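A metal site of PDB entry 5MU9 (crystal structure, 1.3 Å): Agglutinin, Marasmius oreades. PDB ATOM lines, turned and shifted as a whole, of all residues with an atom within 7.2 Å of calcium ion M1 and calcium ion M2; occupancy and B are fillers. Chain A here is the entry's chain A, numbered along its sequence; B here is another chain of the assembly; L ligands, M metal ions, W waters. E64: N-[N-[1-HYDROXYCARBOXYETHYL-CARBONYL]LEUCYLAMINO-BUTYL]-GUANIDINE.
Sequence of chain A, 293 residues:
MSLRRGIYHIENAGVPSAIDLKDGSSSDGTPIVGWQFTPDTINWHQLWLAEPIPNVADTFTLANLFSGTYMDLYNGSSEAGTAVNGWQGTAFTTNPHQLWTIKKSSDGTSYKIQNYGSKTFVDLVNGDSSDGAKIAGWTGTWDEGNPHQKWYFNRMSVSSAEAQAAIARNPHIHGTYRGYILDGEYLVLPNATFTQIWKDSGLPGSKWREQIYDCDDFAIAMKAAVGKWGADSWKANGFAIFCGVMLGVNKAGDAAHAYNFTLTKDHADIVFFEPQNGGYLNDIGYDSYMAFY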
ATOM      1  N   ARG A 209      -7.226  26.432   6.264  1.00  0.00           N
ATOM      2  CA  ARG A 209      -5.977  27.196   6.312  1.00  0.00           C
ATOM      3  C   ARG A 209      -4.933  26.498   5.497  1.00  0.00           C
ATOM      4  O   ARG A 209      -4.715  25.280   5.563  1.00  0.00           O
ATOM      5  CB  ARG A 209      -5.492  27.241   7.788  1.00  0.00           C
ATOM      6  CG  ARG A 209      -6.425  28.026   8.703  1.00  0.00           C
ATOM      7  CD  ARG A 209      -6.077  27.948  10.179  1.00  0.00           C
ATOM      8  NE  ARG A 209      -4.718  28.476  10.397  1.00  0.00           N
ATOM      9  CZ  ARG A 209      -3.997  28.296  11.486  1.00  0.00           C
ATOM     10  NH1 ARG A 209      -4.446  27.623  12.551  1.00  0.00           N
ATOM     11  NH2 ARG A 209      -2.726  28.686  11.495  1.00  0.00           N
ATOM     12  N   GLU A 210      -4.249  27.305   4.622  1.00  0.00           N
ATOM     13  CA  GLU A 210      -3.272  26.756   3.708  1.00  0.00           C
ATOM     14  C   GLU A 210      -2.221  25.876   4.380  1.00  0.00           C
ATOM     15  O   GLU A 210      -1.500  26.353   5.289  1.00  0.00           O
ATOM     16  CB  GLU A 210      -2.613  28.000   3.042  1.00  0.00           C
ATOM     17  CG  GLU A 210      -1.675  27.711   1.941  1.00  0.00           C
ATOM     18  CD  GLU A 210      -0.896  28.955   1.527  1.00  0.00           C
ATOM     19  OE1 GLU A 210      -1.404  30.053   1.621  1.00  0.00           O
ATOM     20  OE2 GLU A 210       0.300  28.809   1.107  1.00  0.00           O
ATOM     21  N   GLN A 211      -2.167  24.608   3.962  1.00  0.00           N
ATOM     22  CA  GLN A 211      -1.312  23.533   4.442  1.00  0.00           C
ATOM     23  C   GLN A 211      -1.538  23.083   5.910  1.00  0.00           C
ATOM     24  O   GLN A 211      -1.560  21.882   6.198  1.00  0.00           O
ATOM     25  CB  GLN A 211       0.191  23.769   4.208  1.00  0.00           C
ATOM     26  CG  GLN A 211       0.535  23.932   2.736  1.00  0.00           C
ATOM     27  CD  GLN A 211       2.045  23.787   2.519  1.00  0.00           C
ATOM     28  OE1 GLN A 211       2.693  22.913   3.006  1.00  0.00           O
ATOM     29  NE2 GLN A 211       2.553  24.641   1.595  1.00  0.00           N
ATOM     30  N   ILE A 212      -1.685  24.075   6.799  1.00  0.00           N
ATOM     31  CA  ILE A 212      -1.740  23.736   8.240  1.00  0.00           C
ATOM     32  C   ILE A 212      -3.102  23.133   8.661  1.00  0.00           C
ATOM     33  O   ILE A 212      -3.176  22.475   9.676  1.00  0.00           O
ATOM     34  CB  ILE A 212      -1.346  25.003   9.027  1.00  0.00           C
ATOM     35  CG1 ILE A 212      -0.961  24.694  10.485  1.00  0.00           C
ATOM     36  CG2 ILE A 212      -2.393  26.118   8.920  1.00  0.00           C
ATOM     37  CD1 ILE A 212       0.265  23.846  10.766  1.00  0.00           C
ATOM     38  N   TYR A 213      -4.141  23.492   7.897  1.00  0.00           N
ATOM     39  CA  TYR A 213      -5.465  22.825   8.139  1.00  0.00           C
ATOM     40  C   TYR A 213      -6.284  22.875   6.880  1.00  0.00           C
ATOM     41  O   TYR A 213      -7.251  23.585   6.797  1.00  0.00           O
ATOM     42  CB  TYR A 213      -6.181  23.316   9.403  1.00  0.00           C
ATOM     43  CG  TYR A 213      -6.908  22.176  10.098  1.00  0.00           C
ATOM     44  CD1 TYR A 213      -6.166  21.238  10.880  1.00  0.00           C
ATOM     45  CD2 TYR A 213      -8.279  21.938   9.963  1.00  0.00           C
ATOM     46  CE1 TYR A 213      -6.767  20.186  11.551  1.00  0.00           C
ATOM     47  CE2 TYR A 213      -8.856  20.845  10.557  1.00  0.00           C
ATOM     48  CZ  TYR A 213      -8.147  19.981  11.337  1.00  0.00           C
ATOM     49  OH  TYR A 213      -8.761  18.860  11.976  1.00  0.00           O
ATOM     50  N   ASP A 214      -5.837  22.038   5.949  1.00  0.00           N
ATOM     51  CA  ASP A 214      -6.408  22.076   4.564  1.00  0.00           C
ATOM     52  C   ASP A 214      -7.056  20.724   4.303  1.00  0.00           C
ATOM     53  O   ASP A 214      -7.398  19.978   5.258  1.00  0.00           O
ATOM     54  CB  ASP A 214      -5.375  22.538   3.538  1.00  0.00           C
ATOM     55  CG  ASP A 214      -4.202  21.578   3.317  1.00  0.00           C
ATOM     56  OD1 ASP A 214      -3.939  20.827   4.269  1.00  0.00           O
ATOM     57  OD2 ASP A 214      -3.582  21.645   2.244  1.00  0.00           O
ATOM     58  N   CYS A 215      -7.366  20.461   3.052  1.00  0.00           N
ATOM     59  CA  CYS A 215      -8.224  19.291   2.734  1.00  0.00           C
ATOM     60  C   CYS A 215      -7.771  17.992   3.364  1.00  0.00           C
ATOM     61  O   CYS A 215      -8.578  17.243   3.922  1.00  0.00           O
ATOM     62  CB  CYS A 215      -8.421  19.159   1.185  1.00  0.00           C
ATOM     63  SG  CYS A 215      -6.816  19.034   0.336  1.00  0.00           S
ATOM     64  N   ASP A 216      -6.477  17.699   3.327  1.00  0.00           N
ATOM     65  CA  ASP A 216      -5.972  16.472   3.850  1.00  0.00           C
ATOM     66  C   ASP A 216      -6.232  16.368   5.401  1.00  0.00           C
ATOM     67  O   ASP A 216      -6.525  15.286   5.932  1.00  0.00           O
ATOM     68  CB  ASP A 216      -4.529  16.212   3.518  1.00  0.00           C
ATOM     69  CG  ASP A 216      -3.672  17.468   3.712  1.00  0.00           C
ATOM     70  OD1 ASP A 216      -3.582  18.244   2.742  1.00  0.00           O
ATOM     71  OD2 ASP A 216      -3.156  17.648   4.863  1.00  0.00           O
ATOM     72  N   ASP A 217      -6.088  17.526   6.085  1.00  0.00           N
ATOM     73  CA  ASP A 217      -6.312  17.504   7.518  1.00  0.00           C
ATOM     74  C   ASP A 217      -7.825  17.242   7.855  1.00  0.00           C
ATOM     75  O   ASP A 217      -8.129  16.462   8.771  1.00  0.00           O
ATOM     76  CB  ASP A 217      -5.956  18.868   8.148  1.00  0.00           C
ATOM     77  CG  ASP A 217      -4.413  19.127   7.955  1.00  0.00           C
ATOM     78  OD1 ASP A 217      -3.665  18.463   8.669  1.00  0.00           O
ATOM     79  OD2 ASP A 217      -4.060  19.830   7.025  1.00  0.00           O
ATOM     80  N   PHE A 218      -8.738  17.862   7.068  1.00  0.00           N
ATOM     81  CA  PHE A 218     -10.153  17.572   7.330  1.00  0.00           C
ATOM     82  C   PHE A 218     -10.462  16.092   7.071  1.00  0.00           C
ATOM     83  O   PHE A 218     -11.207  15.487   7.825  1.00  0.00           O
ATOM     84  CB  PHE A 218     -11.027  18.403   6.436  1.00  0.00           C
ATOM     85  CG  PHE A 218     -11.226  19.845   6.794  1.00  0.00           C
ATOM     86  CD1 PHE A 218     -10.241  20.815   6.537  1.00  0.00           C
ATOM     87  CD2 PHE A 218     -12.387  20.295   7.416  1.00  0.00           C
ATOM     88  CE1 PHE A 218     -10.470  22.151   6.897  1.00  0.00           C
ATOM     89  CE2 PHE A 218     -12.562  21.582   7.857  1.00  0.00           C
ATOM     90  CZ  PHE A 218     -11.609  22.597   7.555  1.00  0.00           C
ATOM     91  N   ALA A 258      -8.465  16.244  -1.208  1.00  0.00           N
ATOM     92  CA  ALA A 258      -8.618  15.163  -0.227  1.00  0.00           C
ATOM     93  C   ALA A 258     -10.016  15.217   0.364  1.00  0.00           C
ATOM     94  O   ALA A 258     -10.458  16.304   0.717  1.00  0.00           O
ATOM     95  CB  ALA A 258      -7.570  15.191   0.819  1.00  0.00           C
ATOM     96  N   ILE B 181       2.095  12.288  -0.883  1.00  0.00           N
ATOM     97  CA  ILE B 181       2.512  13.546  -0.319  1.00  0.00           C
ATOM     98  C   ILE B 181       1.320  14.470  -0.231  1.00  0.00           C
ATOM     99  O   ILE B 181       0.511  14.624  -1.156  1.00  0.00           O
ATOM    100  CB  ILE B 181       3.611  14.214  -1.191  1.00  0.00           C
ATOM    101  CG1 ILE B 181       4.861  13.373  -1.128  1.00  0.00           C
ATOM    102  CG2 ILE B 181       3.834  15.624  -0.757  1.00  0.00           C
ATOM    103  CD1 ILE B 181       5.932  13.848  -2.049  1.00  0.00           C
ATOM    104  N   LEU B 182       1.086  15.017   0.963  1.00  0.00           N
ATOM    105  CA  LEU B 182      -0.107  15.821   1.261  1.00  0.00           C
ATOM    106  C   LEU B 182       0.087  17.311   1.277  1.00  0.00           C
ATOM    107  O   LEU B 182      -0.902  18.111   1.131  1.00  0.00           O
ATOM    108  CB  LEU B 182      -0.749  15.353   2.574  1.00  0.00           C
ATOM    109  CG  LEU B 182      -1.051  13.869   2.628  1.00  0.00           C
ATOM    110  CD1 LEU B 182      -1.470  13.429   4.081  1.00  0.00           C
ATOM    111  CD2 LEU B 182      -2.149  13.443   1.655  1.00  0.00           C
ATOM    112  N   ASP B 183       1.315  17.767   1.663  1.00  0.00           N
ATOM    113  CA  ASP B 183       1.620  19.187   1.877  1.00  0.00           C
ATOM    114  C   ASP B 183       2.958  19.478   1.216  1.00  0.00           C
ATOM    115  O   ASP B 183       3.559  18.610   0.602  1.00  0.00           O
ATOM    116  CB  ASP B 183       1.549  19.608   3.319  1.00  0.00           C
ATOM    117  CG  ASP B 183       0.070  19.405   3.926  1.00  0.00           C
ATOM    118  OD1 ASP B 183      -0.796  20.127   3.384  1.00  0.00           O
ATOM    119  OD2 ASP B 183      -0.031  18.695   4.943  1.00  0.00           O
ATOM    120  N   GLY B 184       3.438  20.686   1.356  1.00  0.00           N
ATOM    121  CA  GLY B 184       4.663  21.184   0.679  1.00  0.00           C
ATOM    122  C   GLY B 184       5.865  21.475   1.570  1.00  0.00           C
ATOM    123  O   GLY B 184       7.005  21.313   1.111  1.00  0.00           O
ATOM    124  N   TYR B 186       7.145  21.353   5.831  1.00  0.00           N
ATOM    125  CA  TYR B 186       6.807  20.705   7.097  1.00  0.00           C
ATOM    126  C   TYR B 186       7.784  21.119   8.238  1.00  0.00           C
ATOM    127  O   TYR B 186       9.000  20.865   8.162  1.00  0.00           O
ATOM    128  CB  TYR B 186       6.887  19.209   6.999  1.00  0.00           C
ATOM    129  CG  TYR B 186       5.970  18.584   5.947  1.00  0.00           C
ATOM    130  CD1 TYR B 186       6.361  18.378   4.670  1.00  0.00           C
ATOM    131  CD2 TYR B 186       4.729  18.135   6.346  1.00  0.00           C
ATOM    132  CE1 TYR B 186       5.542  17.733   3.764  1.00  0.00           C
ATOM    133  CE2 TYR B 186       3.895  17.493   5.456  1.00  0.00           C
ATOM    134  CZ  TYR B 186       4.287  17.273   4.138  1.00  0.00           C
ATOM    135  OH  TYR B 186       3.508  16.549   3.299  1.00  0.00           O
ATOM    136  N   LYS B 223      -1.606  10.740  13.604  1.00  0.00           N
ATOM    137  CA  LYS B 223      -1.459  11.744  12.574  1.00  0.00           C
ATOM    138  C   LYS B 223      -2.505  12.868  12.689  1.00  0.00           C
ATOM    139  O   LYS B 223      -2.235  14.049  12.586  1.00  0.00           O
ATOM    140  CB  LYS B 223      -1.504  11.155  11.187  1.00  0.00           C
ATOM    141  CG  LYS B 223      -1.238  12.208  10.102  1.00  0.00           C
ATOM    142  CD  LYS B 223      -0.770  11.696   8.765  1.00  0.00           C
ATOM    143  CE  LYS B 223      -0.641  12.771   7.718  1.00  0.00           C
ATOM    144  NZ  LYS B 223       0.190  13.907   8.218  1.00  0.00           N
ATOM    145  N   PHE B 239       2.355  26.100   5.867  1.00  0.00           N
ATOM    146  CA  PHE B 239       3.248  24.995   6.199  1.00  0.00           C
ATOM    147  C   PHE B 239       2.390  23.973   6.973  1.00  0.00           C
ATOM    148  O   PHE B 239       1.249  24.276   7.330  1.00  0.00           O
ATOM    149  CB  PHE B 239       4.371  25.484   7.130  1.00  0.00           C
ATOM    150  CG  PHE B 239       3.869  25.972   8.476  1.00  0.00           C
ATOM    151  CD1 PHE B 239       3.162  27.158   8.692  1.00  0.00           C
ATOM    152  CD2 PHE B 239       4.059  25.143   9.541  1.00  0.00           C
ATOM    153  CE1 PHE B 239       2.604  27.436  10.007  1.00  0.00           C
ATOM    154  CE2 PHE B 239       3.608  25.473  10.794  1.00  0.00           C
ATOM    155  CZ  PHE B 239       2.884  26.546  11.033  1.00  0.00           C
ATOM    156  N   ALA B 240       2.900  22.778   7.139  1.00  0.00           N
ATOM    157  CA  ALA B 240       2.286  21.724   7.912  1.00  0.00           C
ATOM    158  C   ALA B 240       3.291  21.190   8.945  1.00  0.00           C
ATOM    159  O   ALA B 240       4.430  21.611   9.002  1.00  0.00           O
ATOM    160  CB  ALA B 240       1.859  20.594   6.928  1.00  0.00           C
ATOM    161  N   ILE B 241       2.848  20.304   9.794  1.00  0.00           N
ATOM    162  CA  ILE B 241       3.651  19.625  10.787  1.00  0.00           C
ATOM    163  C   ILE B 241       4.014  18.242  10.258  1.00  0.00           C
ATOM    164  O   ILE B 241       3.133  17.548   9.787  1.00  0.00           O
ATOM    165  CB  ILE B 241       3.015  19.525  12.130  1.00  0.00           C
ATOM    166  CG1 ILE B 241       2.342  20.821  12.557  1.00  0.00           C
ATOM    167  CG2 ILE B 241       4.000  19.055  13.195  1.00  0.00           C
ATOM    168  CD1 ILE B 241       3.241  22.063  12.586  1.00  0.00           C
ATOM    169  N   TYR B 293       1.896  11.453   4.203  1.00  0.00           N
ATOM    170  CA  TYR B 293       2.486  12.476   5.082  1.00  0.00           C
ATOM    171  C   TYR B 293       2.357  13.790   4.440  1.00  0.00           C
ATOM    172  O   TYR B 293       2.352  14.816   5.159  1.00  0.00           O
ATOM    173  CB  TYR B 293       3.999  12.219   5.275  1.00  0.00           C
ATOM    174  CG  TYR B 293       4.848  12.038   4.073  1.00  0.00           C
ATOM    175  CD1 TYR B 293       4.972  10.798   3.433  1.00  0.00           C
ATOM    176  CD2 TYR B 293       5.537  13.106   3.550  1.00  0.00           C
ATOM    177  CE1 TYR B 293       5.794  10.585   2.319  1.00  0.00           C
ATOM    178  CE2 TYR B 293       6.294  12.932   2.389  1.00  0.00           C
ATOM    179  CZ  TYR B 293       6.464  11.663   1.806  1.00  0.00           C
ATOM    180  OH  TYR B 293       7.270  11.531   0.706  1.00  0.00           O
ATOM    181  OXT TYR B 293       2.261  13.833   3.182  1.00  0.00           O
HETATM  182  C1  E64 L   1      -7.621  21.706  -0.418  1.00  0.00           C
HETATM  183  O1  E64 L   1      -7.437  22.108   0.784  1.00  0.00           O
HETATM  184  O2  E64 L   1      -8.476  22.181  -1.325  1.00  0.00           O
HETATM  185  C2  E64 L   1      -6.706  20.524  -0.881  1.00  0.00           C
HETATM  186  C3  E64 L   1      -5.315  21.099  -0.849  1.00  0.00           C
HETATM  187  O3  E64 L   1      -5.227  21.952  -2.069  1.00  0.00           O
HETATM  188  C4  E64 L   1      -4.296  19.950  -1.094  1.00  0.00           C
HETATM  189  O4  E64 L   1      -3.553  19.453  -0.307  1.00  0.00           O
HETATM  190  N1  E64 L   1      -4.146  19.606  -2.407  1.00  0.00           N
HETATM  191  C6  E64 L   1      -3.074  18.699  -2.744  1.00  0.00           C
HETATM  192  C7  E64 L   1      -3.661  17.281  -3.067  1.00  0.00           C
HETATM  193  C8  E64 L   1      -4.356  16.478  -1.949  1.00  0.00           C
HETATM  194  C9  E64 L   1      -3.462  16.073  -0.858  1.00  0.00           C
HETATM  195  C10 E64 L   1      -4.923  15.228  -2.580  1.00  0.00           C
HETATM  196  C11 E64 L   1      -2.362  19.070  -4.040  1.00  0.00           C
HETATM  197  O5  E64 L   1      -2.978  19.746  -4.835  1.00  0.00           O
HETATM  198  N2  E64 L   1      -1.123  18.586  -4.294  1.00  0.00           N
HETATM  199  C12 E64 L   1      -0.345  18.906  -5.503  1.00  0.00           C
HETATM  200  C13 E64 L   1      -0.209  17.734  -6.453  1.00  0.00           C
HETATM  201  C14 E64 L   1      -0.058  16.376  -5.758  1.00  0.00           C
HETATM  202  C15 E64 L   1      -1.353  15.595  -5.912  1.00  0.00           C
HETATM  203  N3  E64 L   1      -1.667  15.110  -7.272  1.00  0.00           N
HETATM  204  C16 E64 L   1      -1.160  13.943  -7.749  1.00  0.00           C
HETATM  205  N4  E64 L   1      -1.786  13.287  -8.721  1.00  0.00           N
HETATM  206  N5  E64 L   1      -0.104  13.332  -7.190  1.00  0.00           N
HETATM  207 CA    CA M   1      -2.213  19.743   5.514  1.00  0.00          CA
HETATM  208 CA    CA M   2      -2.279  19.809   1.616  1.00  0.00          CA
HETATM  209  O   HOH W   1      -1.305  18.762   7.559  1.00  0.00           O
HETATM  210  O   HOH W   2      -0.986  21.265   0.264  1.00  0.00           O
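The side-chain sulfur (SG) of Cys 215 is covalently linked to a carbon (C2) of the ligand (1.9 Å). O1 of the ligand is in hydrogen-bond range of N of Cys 215, 2.8 Å away.
OH of Tyr 186 of chain B lies within hydrogen-bond range of N of Asp 183 of chain B. O of Arg 209 sits at hydrogen-bond distance from N of Asp 214. The backbone NH of Leu 182 of chain B lies within hydrogen-bond range of the chain-end carboxylate of Tyr 293 of chain B (2.8 Å). The side-chain amide oxygen (OE1) of Gln 211 is in hydrogen-bond range of the backbone NH (N) of Gly 184 of chain B.
Five residues have an atom within 4 Å of calcium ion M1: Gln 211, Asp 214, Asp 216, Asp 217 and Asp 183 of chain B.
Of the 21 residues printed, 4 come within 4 Å of calcium ion M2.
Calcium ion M1 is bound by the backbone carbonyl oxygen (O) of Gln 211 (2.3 Å), the side-chain carboxylate (OD2) of Asp 216 (2.4 Å), the side-chain carboxylate (OD2) of Asp 217 (2.4 Å), the side-chain carboxylate (OD1) of Asp 214 (2.4 Å), water W1 (2.4 Å), the side-chain carboxylate (OD2) of Asp 183 of chain B (2.5 Å) and the side-chain carboxylate (OD1) of Asp 183 of chain B (2.6 Å). Calcium ion M1 has seven donor atoms within binding distance.
Calcium ion M2 is bound by the backbone carbonyl oxygen (O) of Leu 182 of chain B (2.2 Å), the side-chain carboxylate (OD1) of Asp 216 (2.3 Å), the side-chain carboxylate (OD1) of Asp 183 of chain B (2.3 Å), an oxygen (O4) of the ligand (2.3 Å), the side-chain carboxylate (OD2) of Asp 214 (2.3 Å) and water W2 (2.4 Å).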
